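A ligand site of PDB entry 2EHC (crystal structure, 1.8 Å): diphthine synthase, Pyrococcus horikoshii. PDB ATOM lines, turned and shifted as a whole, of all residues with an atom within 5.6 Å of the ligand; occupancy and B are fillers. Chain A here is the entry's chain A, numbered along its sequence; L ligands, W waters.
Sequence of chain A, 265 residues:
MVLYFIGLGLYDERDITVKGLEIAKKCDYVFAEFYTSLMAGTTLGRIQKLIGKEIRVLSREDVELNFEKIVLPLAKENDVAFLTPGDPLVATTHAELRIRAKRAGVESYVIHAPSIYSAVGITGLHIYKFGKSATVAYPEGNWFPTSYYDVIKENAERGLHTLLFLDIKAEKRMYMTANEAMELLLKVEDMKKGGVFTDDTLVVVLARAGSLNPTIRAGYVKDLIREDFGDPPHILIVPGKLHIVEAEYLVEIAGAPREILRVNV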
ATOM      1  N   LEU A  10      -0.895  16.187 -19.624  1.00  0.00           N
ATOM      2  CA  LEU A  10      -1.316  16.478 -18.249  1.00  0.00           C
ATOM      3  C   LEU A  10      -0.739  17.601 -17.409  1.00  0.00           C
ATOM      4  O   LEU A  10      -1.498  18.302 -16.728  1.00  0.00           O
ATOM      5  CB  LEU A  10      -1.161  15.207 -17.427  1.00  0.00           C
ATOM      6  CG  LEU A  10      -1.863  13.935 -17.912  1.00  0.00           C
ATOM      7  CD1 LEU A  10      -1.198  12.717 -17.301  1.00  0.00           C
ATOM      8  CD2 LEU A  10      -3.331  13.993 -17.554  1.00  0.00           C
ATOM      9  N   TYR A  11       0.575  17.777 -17.431  1.00  0.00           N
ATOM     10  CA  TYR A  11       1.202  18.733 -16.533  1.00  0.00           C
ATOM     11  C   TYR A  11       2.207  19.730 -17.099  1.00  0.00           C
ATOM     12  O   TYR A  11       2.123  20.921 -16.817  1.00  0.00           O
ATOM     13  CB  TYR A  11       1.866  17.903 -15.423  1.00  0.00           C
ATOM     14  CG  TYR A  11       2.513  18.688 -14.305  1.00  0.00           C
ATOM     15  CD1 TYR A  11       1.742  19.387 -13.379  1.00  0.00           C
ATOM     16  CD2 TYR A  11       3.892  18.686 -14.156  1.00  0.00           C
ATOM     17  CE1 TYR A  11       2.338  20.075 -12.314  1.00  0.00           C
ATOM     18  CE2 TYR A  11       4.511  19.361 -13.103  1.00  0.00           C
ATOM     19  CZ  TYR A  11       3.726  20.055 -12.196  1.00  0.00           C
ATOM     20  OH  TYR A  11       4.325  20.710 -11.155  1.00  0.00           O
ATOM     21  N   THR A  36      -9.646  24.969 -21.279  1.00  0.00           N
ATOM     22  CA  THR A  36     -10.309  23.707 -20.981  1.00  0.00           C
ATOM     23  C   THR A  36      -9.672  22.958 -19.812  1.00  0.00           C
ATOM     24  O   THR A  36     -10.290  22.088 -19.200  1.00  0.00           O
ATOM     25  CB  THR A  36     -10.332  22.754 -22.201  1.00  0.00           C
ATOM     26  OG1 THR A  36      -9.005  22.535 -22.674  1.00  0.00           O
ATOM     27  CG2 THR A  36     -11.181  23.348 -23.310  1.00  0.00           C
ATOM     28  N   SER A  37      -8.423  23.288 -19.508  1.00  0.00           N
ATOM     29  CA  SER A  37      -7.733  22.659 -18.400  1.00  0.00           C
ATOM     30  C   SER A  37      -6.536  23.499 -17.977  1.00  0.00           C
ATOM     31  O   SER A  37      -6.236  24.526 -18.586  1.00  0.00           O
ATOM     32  CB  SER A  37      -7.263  21.251 -18.779  1.00  0.00           C
ATOM     33  OG  SER A  37      -6.772  20.566 -17.634  1.00  0.00           O
ATOM     34  N   LEU A  38      -5.845  23.045 -16.927  1.00  0.00           N
ATOM     35  CA  LEU A  38      -4.682  23.746 -16.413  1.00  0.00           C
ATOM     36  C   LEU A  38      -3.434  22.872 -16.416  1.00  0.00           C
ATOM     37  O   LEU A  38      -3.422  21.791 -15.826  1.00  0.00           O
ATOM     38  CB  LEU A  38      -4.941  24.239 -14.991  1.00  0.00           C
ATOM     39  CG  LEU A  38      -3.738  24.824 -14.254  1.00  0.00           C
ATOM     40  CD1 LEU A  38      -3.357  26.171 -14.871  1.00  0.00           C
ATOM     41  CD2 LEU A  38      -4.068  24.999 -12.771  1.00  0.00           C
ATOM     42  N   PRO A  85      -4.612  21.439 -23.729  1.00  0.00           N
ATOM     43  CA  PRO A  85      -4.045  20.684 -22.598  1.00  0.00           C
ATOM     44  C   PRO A  85      -4.624  19.271 -22.684  1.00  0.00           C
ATOM     45  O   PRO A  85      -5.666  19.071 -23.318  1.00  0.00           O
ATOM     46  CB  PRO A  85      -4.582  21.433 -21.379  1.00  0.00           C
ATOM     47  CG  PRO A  85      -4.797  22.830 -21.888  1.00  0.00           C
ATOM     48  CD  PRO A  85      -5.392  22.598 -23.252  1.00  0.00           C
ATOM     49  N   GLY A  86      -3.961  18.314 -22.046  1.00  0.00           N
ATOM     50  CA  GLY A  86      -4.437  16.929 -22.053  1.00  0.00           C
ATOM     51  C   GLY A  86      -4.705  16.397 -23.440  1.00  0.00           C
ATOM     52  O   GLY A  86      -3.917  16.631 -24.357  1.00  0.00           O
ATOM     53  N   ASP A  87      -5.783  15.641 -23.591  1.00  0.00           N
ATOM     54  CA  ASP A  87      -6.173  15.112 -24.899  1.00  0.00           C
ATOM     55  C   ASP A  87      -7.199  16.119 -25.416  1.00  0.00           C
ATOM     56  O   ASP A  87      -8.139  16.483 -24.726  1.00  0.00           O
ATOM     57  CB  ASP A  87      -6.815  13.727 -24.748  1.00  0.00           C
ATOM     58  CG  ASP A  87      -7.179  13.105 -26.085  1.00  0.00           C
ATOM     59  OD1 ASP A  87      -8.122  13.599 -26.731  1.00  0.00           O
ATOM     60  OD2 ASP A  87      -6.506  12.137 -26.509  1.00  0.00           O
ATOM     61  N   PRO A  88      -7.019  16.568 -26.669  1.00  0.00           N
ATOM     62  CA  PRO A  88      -7.938  17.559 -27.244  1.00  0.00           C
ATOM     63  C   PRO A  88      -9.424  17.216 -27.332  1.00  0.00           C
ATOM     64  O   PRO A  88     -10.254  18.133 -27.387  1.00  0.00           O
ATOM     65  CB  PRO A  88      -7.332  17.827 -28.615  1.00  0.00           C
ATOM     66  CG  PRO A  88      -6.714  16.512 -28.981  1.00  0.00           C
ATOM     67  CD  PRO A  88      -6.073  16.081 -27.679  1.00  0.00           C
ATOM     68  N   LEU A  89      -9.764  15.934 -27.328  1.00  0.00           N
ATOM     69  CA  LEU A  89     -11.172  15.533 -27.459  1.00  0.00           C
ATOM     70  C   LEU A  89     -11.795  14.897 -26.236  1.00  0.00           C
ATOM     71  O   LEU A  89     -12.834  14.244 -26.329  1.00  0.00           O
ATOM     72  CB  LEU A  89     -11.312  14.572 -28.650  1.00  0.00           C
ATOM     73  CG  LEU A  89     -10.726  15.057 -29.971  1.00  0.00           C
ATOM     74  CD1 LEU A  89     -11.058  14.061 -31.065  1.00  0.00           C
ATOM     75  CD2 LEU A  89     -11.278  16.432 -30.305  1.00  0.00           C
ATOM     76  N   VAL A  90     -11.166  15.075 -25.076  1.00  0.00           N
ATOM     77  CA  VAL A  90     -11.678  14.515 -23.836  1.00  0.00           C
ATOM     78  C   VAL A  90     -12.232  15.613 -22.928  1.00  0.00           C
ATOM     79  O   VAL A  90     -11.486  16.482 -22.478  1.00  0.00           O
ATOM     80  CB  VAL A  90     -10.583  13.745 -23.067  1.00  0.00           C
ATOM     81  CG1 VAL A  90     -11.077  13.368 -21.679  1.00  0.00           C
ATOM     82  CG2 VAL A  90     -10.187  12.494 -23.842  1.00  0.00           C
ATOM     83  N   ALA A  91     -13.539  15.569 -22.663  1.00  0.00           N
ATOM     84  CA  ALA A  91     -14.176  16.547 -21.786  1.00  0.00           C
ATOM     85  C   ALA A  91     -14.025  17.974 -22.310  1.00  0.00           C
ATOM     86  O   ALA A  91     -13.841  18.925 -21.541  1.00  0.00           O
ATOM     87  CB  ALA A  91     -13.635  16.424 -20.368  1.00  0.00           C
ATOM     88  N   THR A  92     -14.077  18.107 -23.620  1.00  0.00           N
ATOM     89  CA  THR A  92     -14.087  19.360 -24.314  1.00  0.00           C
ATOM     90  C   THR A  92     -15.143  19.219 -25.374  1.00  0.00           C
ATOM     91  O   THR A  92     -15.668  18.137 -25.588  1.00  0.00           O
ATOM     92  CB  THR A  92     -12.722  19.610 -24.994  1.00  0.00           C
ATOM     93  OG1 THR A  92     -12.601  18.809 -26.158  1.00  0.00           O
ATOM     94  CG2 THR A  92     -11.539  19.329 -24.054  1.00  0.00           C
ATOM     95  N   PRO A 114      -1.569  12.188 -23.082  1.00  0.00           N
ATOM     96  CA  PRO A 114      -2.127  11.659 -21.829  1.00  0.00           C
ATOM     97  C   PRO A 114      -3.281  12.520 -21.319  1.00  0.00           C
ATOM     98  O   PRO A 114      -3.224  13.753 -21.336  1.00  0.00           O
ATOM     99  CB  PRO A 114      -0.919  11.640 -20.880  1.00  0.00           C
ATOM    100  CG  PRO A 114       0.191  12.456 -21.496  1.00  0.00           C
ATOM    101  CD  PRO A 114      -0.116  12.429 -22.967  1.00  0.00           C
ATOM    102  N   SER A 115      -4.347  11.842 -20.897  1.00  0.00           N
ATOM    103  CA  SER A 115      -5.564  12.500 -20.420  1.00  0.00           C
ATOM    104  C   SER A 115      -5.842  12.144 -18.975  1.00  0.00           C
ATOM    105  O   SER A 115      -5.509  11.048 -18.525  1.00  0.00           O
ATOM    106  CB  SER A 115      -6.747  12.069 -21.294  1.00  0.00           C
ATOM    107  OG  SER A 115      -7.976  12.543 -20.769  1.00  0.00           O
ATOM    108  N   ILE A 116      -6.463  13.062 -18.244  1.00  0.00           N
ATOM    109  CA  ILE A 116      -6.784  12.798 -16.854  1.00  0.00           C
ATOM    110  C   ILE A 116      -7.783  11.648 -16.750  1.00  0.00           C
ATOM    111  O   ILE A 116      -7.815  10.922 -15.758  1.00  0.00           O
ATOM    112  CB  ILE A 116      -7.379  14.056 -16.174  1.00  0.00           C
ATOM    113  CG1 ILE A 116      -7.525  13.816 -14.670  1.00  0.00           C
ATOM    114  CG2 ILE A 116      -8.722  14.402 -16.792  1.00  0.00           C
ATOM    115  CD1 ILE A 116      -6.203  13.541 -13.965  1.00  0.00           C
ATOM    116  N   TYR A 117      -8.579  11.460 -17.811  1.00  0.00           N
ATOM    117  CA  TYR A 117      -9.586  10.407 -17.846  1.00  0.00           C
ATOM    118  C   TYR A 117      -8.977   9.016 -17.666  1.00  0.00           C
ATOM    119  O   TYR A 117      -9.567   8.146 -17.019  1.00  0.00           O
ATOM    120  CB  TYR A 117     -10.356  10.514 -19.173  1.00  0.00           C
ATOM    121  CG  TYR A 117     -11.492   9.523 -19.359  1.00  0.00           C
ATOM    122  CD1 TYR A 117     -12.592   9.512 -18.493  1.00  0.00           C
ATOM    123  CD2 TYR A 117     -11.478   8.634 -20.425  1.00  0.00           C
ATOM    124  CE1 TYR A 117     -13.654   8.630 -18.705  1.00  0.00           C
ATOM    125  CE2 TYR A 117     -12.519   7.748 -20.644  1.00  0.00           C
ATOM    126  CZ  TYR A 117     -13.613   7.751 -19.786  1.00  0.00           C
ATOM    127  OH  TYR A 117     -14.654   6.886 -20.031  1.00  0.00           O
ATOM    128  N   LEU A 164     -15.084  12.696 -11.139  1.00  0.00           N
ATOM    129  CA  LEU A 164     -15.663  14.028 -11.130  1.00  0.00           C
ATOM    130  C   LEU A 164     -14.658  15.086 -11.575  1.00  0.00           C
ATOM    131  O   LEU A 164     -13.715  15.431 -10.851  1.00  0.00           O
ATOM    132  CB  LEU A 164     -16.172  14.369  -9.723  1.00  0.00           C
ATOM    133  CG  LEU A 164     -17.271  13.465  -9.153  1.00  0.00           C
ATOM    134  CD1 LEU A 164     -17.452  13.724  -7.660  1.00  0.00           C
ATOM    135  CD2 LEU A 164     -18.570  13.737  -9.899  1.00  0.00           C
ATOM    136  N   PHE A 165     -14.836  15.569 -12.802  1.00  0.00           N
ATOM    137  CA  PHE A 165     -14.007  16.627 -13.341  1.00  0.00           C
ATOM    138  C   PHE A 165     -14.402  17.832 -12.506  1.00  0.00           C
ATOM    139  O   PHE A 165     -15.575  17.968 -12.149  1.00  0.00           O
ATOM    140  CB  PHE A 165     -14.369  16.883 -14.806  1.00  0.00           C
ATOM    141  CG  PHE A 165     -14.005  15.768 -15.743  1.00  0.00           C
ATOM    142  CD1 PHE A 165     -12.713  15.667 -16.252  1.00  0.00           C
ATOM    143  CD2 PHE A 165     -14.952  14.831 -16.128  1.00  0.00           C
ATOM    144  CE1 PHE A 165     -12.370  14.638 -17.142  1.00  0.00           C
ATOM    145  CE2 PHE A 165     -14.618  13.800 -17.016  1.00  0.00           C
ATOM    146  CZ  PHE A 165     -13.328  13.708 -17.521  1.00  0.00           C
ATOM    147  N   LEU A 166     -13.454  18.709 -12.187  1.00  0.00           N
ATOM    148  CA  LEU A 166     -13.769  19.898 -11.391  1.00  0.00           C
ATOM    149  C   LEU A 166     -13.753  21.152 -12.268  1.00  0.00           C
ATOM    150  O   LEU A 166     -13.015  21.230 -13.249  1.00  0.00           O
ATOM    151  CB  LEU A 166     -12.781  20.012 -10.234  1.00  0.00           C
ATOM    152  CG  LEU A 166     -12.733  18.756  -9.354  1.00  0.00           C
ATOM    153  CD1 LEU A 166     -11.867  19.008  -8.125  1.00  0.00           C
ATOM    154  CD2 LEU A 166     -14.146  18.368  -8.918  1.00  0.00           C
ATOM    155  N   ASP A 167     -14.585  22.121 -11.909  1.00  0.00           N
ATOM    156  CA  ASP A 167     -14.723  23.348 -12.697  1.00  0.00           C
ATOM    157  C   ASP A 167     -13.474  24.202 -12.833  1.00  0.00           C
ATOM    158  O   ASP A 167     -12.555  24.146 -12.014  1.00  0.00           O
ATOM    159  CB  ASP A 167     -15.871  24.188 -12.131  1.00  0.00           C
ATOM    160  CG  ASP A 167     -16.552  25.040 -13.195  1.00  0.00           C
ATOM    161  OD1 ASP A 167     -16.137  24.985 -14.375  1.00  0.00           O
ATOM    162  OD2 ASP A 167     -17.519  25.758 -12.855  1.00  0.00           O
ATOM    163  N   ILE A 168     -13.450  24.988 -13.900  1.00  0.00           N
ATOM    164  CA  ILE A 168     -12.344  25.887 -14.178  1.00  0.00           C
ATOM    165  C   ILE A 168     -12.855  27.146 -14.861  1.00  0.00           C
ATOM    166  O   ILE A 168     -13.688  27.082 -15.758  1.00  0.00           O
ATOM    167  CB  ILE A 168     -11.281  25.205 -15.092  1.00  0.00           C
ATOM    168  CG1 ILE A 168     -10.222  26.238 -15.507  1.00  0.00           C
ATOM    169  CG2 ILE A 168     -11.953  24.614 -16.321  1.00  0.00           C
ATOM    170  CD1 ILE A 168      -9.075  25.668 -16.339  1.00  0.00           C
ATOM    171  N   LEU A 206      -6.844  13.216  -6.698  1.00  0.00           N
ATOM    172  CA  LEU A 206      -5.642  13.141  -7.524  1.00  0.00           C
ATOM    173  C   LEU A 206      -5.344  14.561  -7.949  1.00  0.00           C
ATOM    174  O   LEU A 206      -6.144  15.197  -8.651  1.00  0.00           O
ATOM    175  CB  LEU A 206      -5.873  12.260  -8.760  1.00  0.00           C
ATOM    176  CG  LEU A 206      -4.697  12.202  -9.748  1.00  0.00           C
ATOM    177  CD1 LEU A 206      -3.422  11.725  -9.046  1.00  0.00           C
ATOM    178  CD2 LEU A 206      -5.056  11.269 -10.901  1.00  0.00           C
ATOM    179  N   ALA A 207      -4.198  15.085  -7.515  1.00  0.00           N
ATOM    180  CA  ALA A 207      -3.817  16.450  -7.851  1.00  0.00           C
ATOM    181  C   ALA A 207      -2.522  16.488  -8.652  1.00  0.00           C
ATOM    182  O   ALA A 207      -1.537  15.842  -8.291  1.00  0.00           O
ATOM    183  CB  ALA A 207      -3.668  17.268  -6.571  1.00  0.00           C
ATOM    184  N   ARG A 208      -2.561  17.253  -9.742  1.00  0.00           N
ATOM    185  CA  ARG A 208      -1.420  17.439 -10.623  1.00  0.00           C
ATOM    186  C   ARG A 208      -0.884  16.141 -11.224  1.00  0.00           C
ATOM    187  O   ARG A 208       0.316  15.842 -11.162  1.00  0.00           O
ATOM    188  CB  ARG A 208      -0.304  18.190  -9.869  1.00  0.00           C
ATOM    189  CG  ARG A 208      -0.750  19.548  -9.327  1.00  0.00           C
ATOM    190  CD  ARG A 208       0.345  20.209  -8.467  1.00  0.00           C
ATOM    191  NE  ARG A 208       0.872  19.270  -7.489  1.00  0.00           N
ATOM    192  CZ  ARG A 208       0.212  18.864  -6.393  1.00  0.00           C
ATOM    193  NH1 ARG A 208      -0.995  19.336  -6.128  1.00  0.00           N
ATOM    194  NH2 ARG A 208       0.759  17.956  -5.596  1.00  0.00           N
ATOM    195  N   ALA A 209      -1.799  15.358 -11.793  1.00  0.00           N
ATOM    196  CA  ALA A 209      -1.412  14.114 -12.453  1.00  0.00           C
ATOM    197  C   ALA A 209      -0.458  14.541 -13.569  1.00  0.00           C
ATOM    198  O   ALA A 209      -0.602  15.632 -14.129  1.00  0.00           O
ATOM    199  CB  ALA A 209      -2.644  13.428 -13.030  1.00  0.00           C
ATOM    200  N   GLY A 210       0.500  13.687 -13.900  1.00  0.00           N
ATOM    201  CA  GLY A 210       1.445  14.039 -14.941  1.00  0.00           C
ATOM    202  C   GLY A 210       2.767  14.490 -14.341  1.00  0.00           C
ATOM    203  O   GLY A 210       3.828  14.249 -14.912  1.00  0.00           O
ATOM    204  N   PRO A 233      -4.246  21.582 -10.970  1.00  0.00           N
ATOM    205  CA  PRO A 233      -5.616  21.075 -10.984  1.00  0.00           C
ATOM    206  C   PRO A 233      -5.849  19.846 -10.114  1.00  0.00           C
ATOM    207  O   PRO A 233      -4.915  19.089  -9.822  1.00  0.00           O
ATOM    208  CB  PRO A 233      -5.843  20.781 -12.462  1.00  0.00           C
ATOM    209  CG  PRO A 233      -4.506  20.277 -12.897  1.00  0.00           C
ATOM    210  CD  PRO A 233      -3.542  21.246 -12.231  1.00  0.00           C
ATOM    211  N   HIS A 234      -7.093  19.664  -9.697  1.00  0.00           N
ATOM    212  CA  HIS A 234      -7.495  18.537  -8.875  1.00  0.00           C
ATOM    213  C   HIS A 234      -8.658  17.827  -9.557  1.00  0.00           C
ATOM    214  O   HIS A 234      -9.392  18.421 -10.347  1.00  0.00           O
ATOM    215  CB  HIS A 234      -8.046  18.976  -7.510  1.00  0.00           C
ATOM    216  CG  HIS A 234      -7.056  19.664  -6.622  1.00  0.00           C
ATOM    217  ND1 HIS A 234      -7.390  20.121  -5.356  1.00  0.00           N
ATOM    218  CD2 HIS A 234      -5.754  19.986  -6.797  1.00  0.00           C
ATOM    219  CE1 HIS A 234      -6.335  20.691  -4.803  1.00  0.00           C
ATOM    220  NE2 HIS A 234      -5.330  20.630  -5.656  1.00  0.00           N
ATOM    221  N   ILE A 235      -8.830  16.550  -9.226  1.00  0.00           N
ATOM    222  CA  ILE A 235      -9.957  15.795  -9.726  1.00  0.00           C
ATOM    223  C   ILE A 235     -10.396  14.992  -8.504  1.00  0.00           C
ATOM    224  O   ILE A 235      -9.567  14.605  -7.678  1.00  0.00           O
ATOM    225  CB  ILE A 235      -9.577  14.884 -10.925  1.00  0.00           C
ATOM    226  CG1 ILE A 235     -10.837  14.569 -11.736  1.00  0.00           C
ATOM    227  CG2 ILE A 235      -8.893  13.610 -10.439  1.00  0.00           C
ATOM    228  CD1 ILE A 235     -10.587  14.425 -13.219  1.00  0.00           C
HETATM  229  N1  LIG L   1      -9.010  17.292 -22.228  1.00  0.00           N
HETATM  230  C1  LIG L   1      -8.506  17.290 -20.801  1.00  0.00           C
HETATM  231  C2  LIG L   1      -9.536  17.476 -19.721  1.00  0.00           C
HETATM  232  C3  LIG L   1     -10.386  18.728 -19.751  1.00  0.00           C
HETATM  233  S1  LIG L   1     -11.409  18.725 -18.223  1.00  0.00           S
HETATM  234  C4  LIG L   1      -7.730  15.924 -20.593  1.00  0.00           C
HETATM  235  O1  LIG L   1      -7.679  15.114 -21.543  1.00  0.00           O
HETATM  236  O2  LIG L   1      -7.183  15.740 -19.429  1.00  0.00           O
HETATM  237  C5  LIG L   1     -10.339  19.650 -17.187  1.00  0.00           C
HETATM  238  C6  LIG L   1     -10.482  19.170 -15.681  1.00  0.00           C
HETATM  239  O3  LIG L   1      -9.899  17.847 -15.601  1.00  0.00           O
HETATM  240  C7  LIG L   1      -9.756  20.005 -14.688  1.00  0.00           C
HETATM  241  O4  LIG L   1     -10.565  21.085 -14.242  1.00  0.00           O
HETATM  242  C8  LIG L   1      -9.401  18.954 -13.603  1.00  0.00           C
HETATM  243  O5  LIG L   1     -10.498  18.718 -12.719  1.00  0.00           O
HETATM  244  C9  LIG L   1      -9.003  17.715 -14.407  1.00  0.00           C
HETATM  245  N2  LIG L   1      -7.705  17.659 -14.781  1.00  0.00           N
HETATM  246  C10 LIG L   1      -7.011  17.895 -15.957  1.00  0.00           C
HETATM  247  N3  LIG L   1      -5.724  17.711 -15.902  1.00  0.00           N
HETATM  248  C11 LIG L   1      -5.498  17.300 -14.564  1.00  0.00           C
HETATM  249  C12 LIG L   1      -4.283  16.937 -13.871  1.00  0.00           C
HETATM  250  N4  LIG L   1      -3.069  16.936 -14.443  1.00  0.00           N
HETATM  251  N5  LIG L   1      -4.448  16.580 -12.545  1.00  0.00           N
HETATM  252  C13 LIG L   1      -5.660  16.572 -11.922  1.00  0.00           C
HETATM  253  N6  LIG L   1      -6.836  16.913 -12.546  1.00  0.00           N
HETATM  254  C14 LIG L   1      -6.677  17.264 -13.860  1.00  0.00           C
HETATM  255  O   HOH W   1      -8.208  19.975 -22.435  1.00  0.00           O
HETATM  256  O   HOH W   2      -5.053  17.366 -18.551  1.00  0.00           O
HETATM  257  O   HOH W   3      -4.273  19.746 -18.223  1.00  0.00           O
HETATM  258  O   HOH W   4      -9.838  23.168 -12.423  1.00  0.00           O
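The backbone carbonyl oxygen (O) of Thr 36 lies close to a sulfur (S1) of the ligand (3.7 Å). N3 of the ligand lies close to OG of Ser 37 (3.5 Å). Pro 85 touches the ligand. Gly 86 touches the ligand (CA to C4, 3.7 Å). Ala 91 touches the ligand (CB to S1, 3.9 Å). Thr 92 touches the ligand (CG2 to N1, 3.7 Å). Phe 165 touches the ligand (CD1 to O3, 3.6 Å). Leu 206 touches the ligand (O to C13, 3.6 Å). Pro 233 touches the ligand (O to C13, 3.4 Å). CB of Ile 235 touches N6 of the ligand, 3.8 Å away. 19 residues have an atom within 4 Å of the ligand: Leu 10, Thr 36, Ser 37, Pro 85, Gly 86, Asp 87, Val 90, Ala 91, Thr 92, Ser 115, Ile 116, Phe 165, Leu 166, Leu 206, Arg 208, Ala 209, Pro 233, His 234 and Ile 235.
The backbone NH (N) of Arg 208 sits at hydrogen-bond distance from a nitrogen (N5) of the ligand (3.4 Å). N5 of the ligand is in hydrogen-bond range of N of Ala 209 (3.0 Å). The backbone carbonyl oxygen (O) of Val 90 is in hydrogen-bond range of a nitrogen (N1) of the ligand, 2.6 Å away. The backbone NH (N) of Asp 87 is in hydrogen-bond range of an oxygen (O1) of the ligand. O of Ala 209 sits at hydrogen-bond distance from N4 of the ligand (2.8 Å). O of Leu 166 sits at hydrogen-bond distance from O4 of the ligand (2.6 Å). O of Asp 87 is in hydrogen-bond range of N1 of the ligand (2.8 Å). An oxygen (O2) of the ligand lies within hydrogen-bond range of the backbone NH (N) of Ile 116, at 3.0 Å. The backbone NH of Leu 166 lies within hydrogen-bond range of an oxygen (O5) of the ligand, at 3.0 Å. O of Leu 10 lies within hydrogen-bond range of N4 of the ligand, at 3.1 Å. An oxygen (O5) of the ligand is in hydrogen-bond range of the backbone carbonyl oxygen (O) of His 234. OG of Ser 115 is in hydrogen-bond range of O1 of the ligand, at 2.7 Å.
The backbone NH (N) of Tyr 117 lies close to the side-chain hydroxyl (OG) of Ser 115. O of Pro 233 sits at hydrogen-bond distance from N of Arg 208 (3.0 Å). The backbone NH (N) of Leu 89 lies within hydrogen-bond range of the side-chain carboxylate (OD1) of Asp 87, 2.9 Å away. O of Leu 206 lies within hydrogen-bond range of N of Ile 235, at 3.1 Å. The side-chain hydroxyl (OG1) of Thr 92 lies within hydrogen-bond range of the backbone carbonyl oxygen (O) of Pro 88 (2.7 Å).
Water W1 lies within hydrogen-bond range of OG1 of Thr 36 (2.7 Å), N1 of the ligand (2.8 Å) and O of Pro 85 (2.8 Å). Water W4 bridges O4 of the ligand and O of Asp 167.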
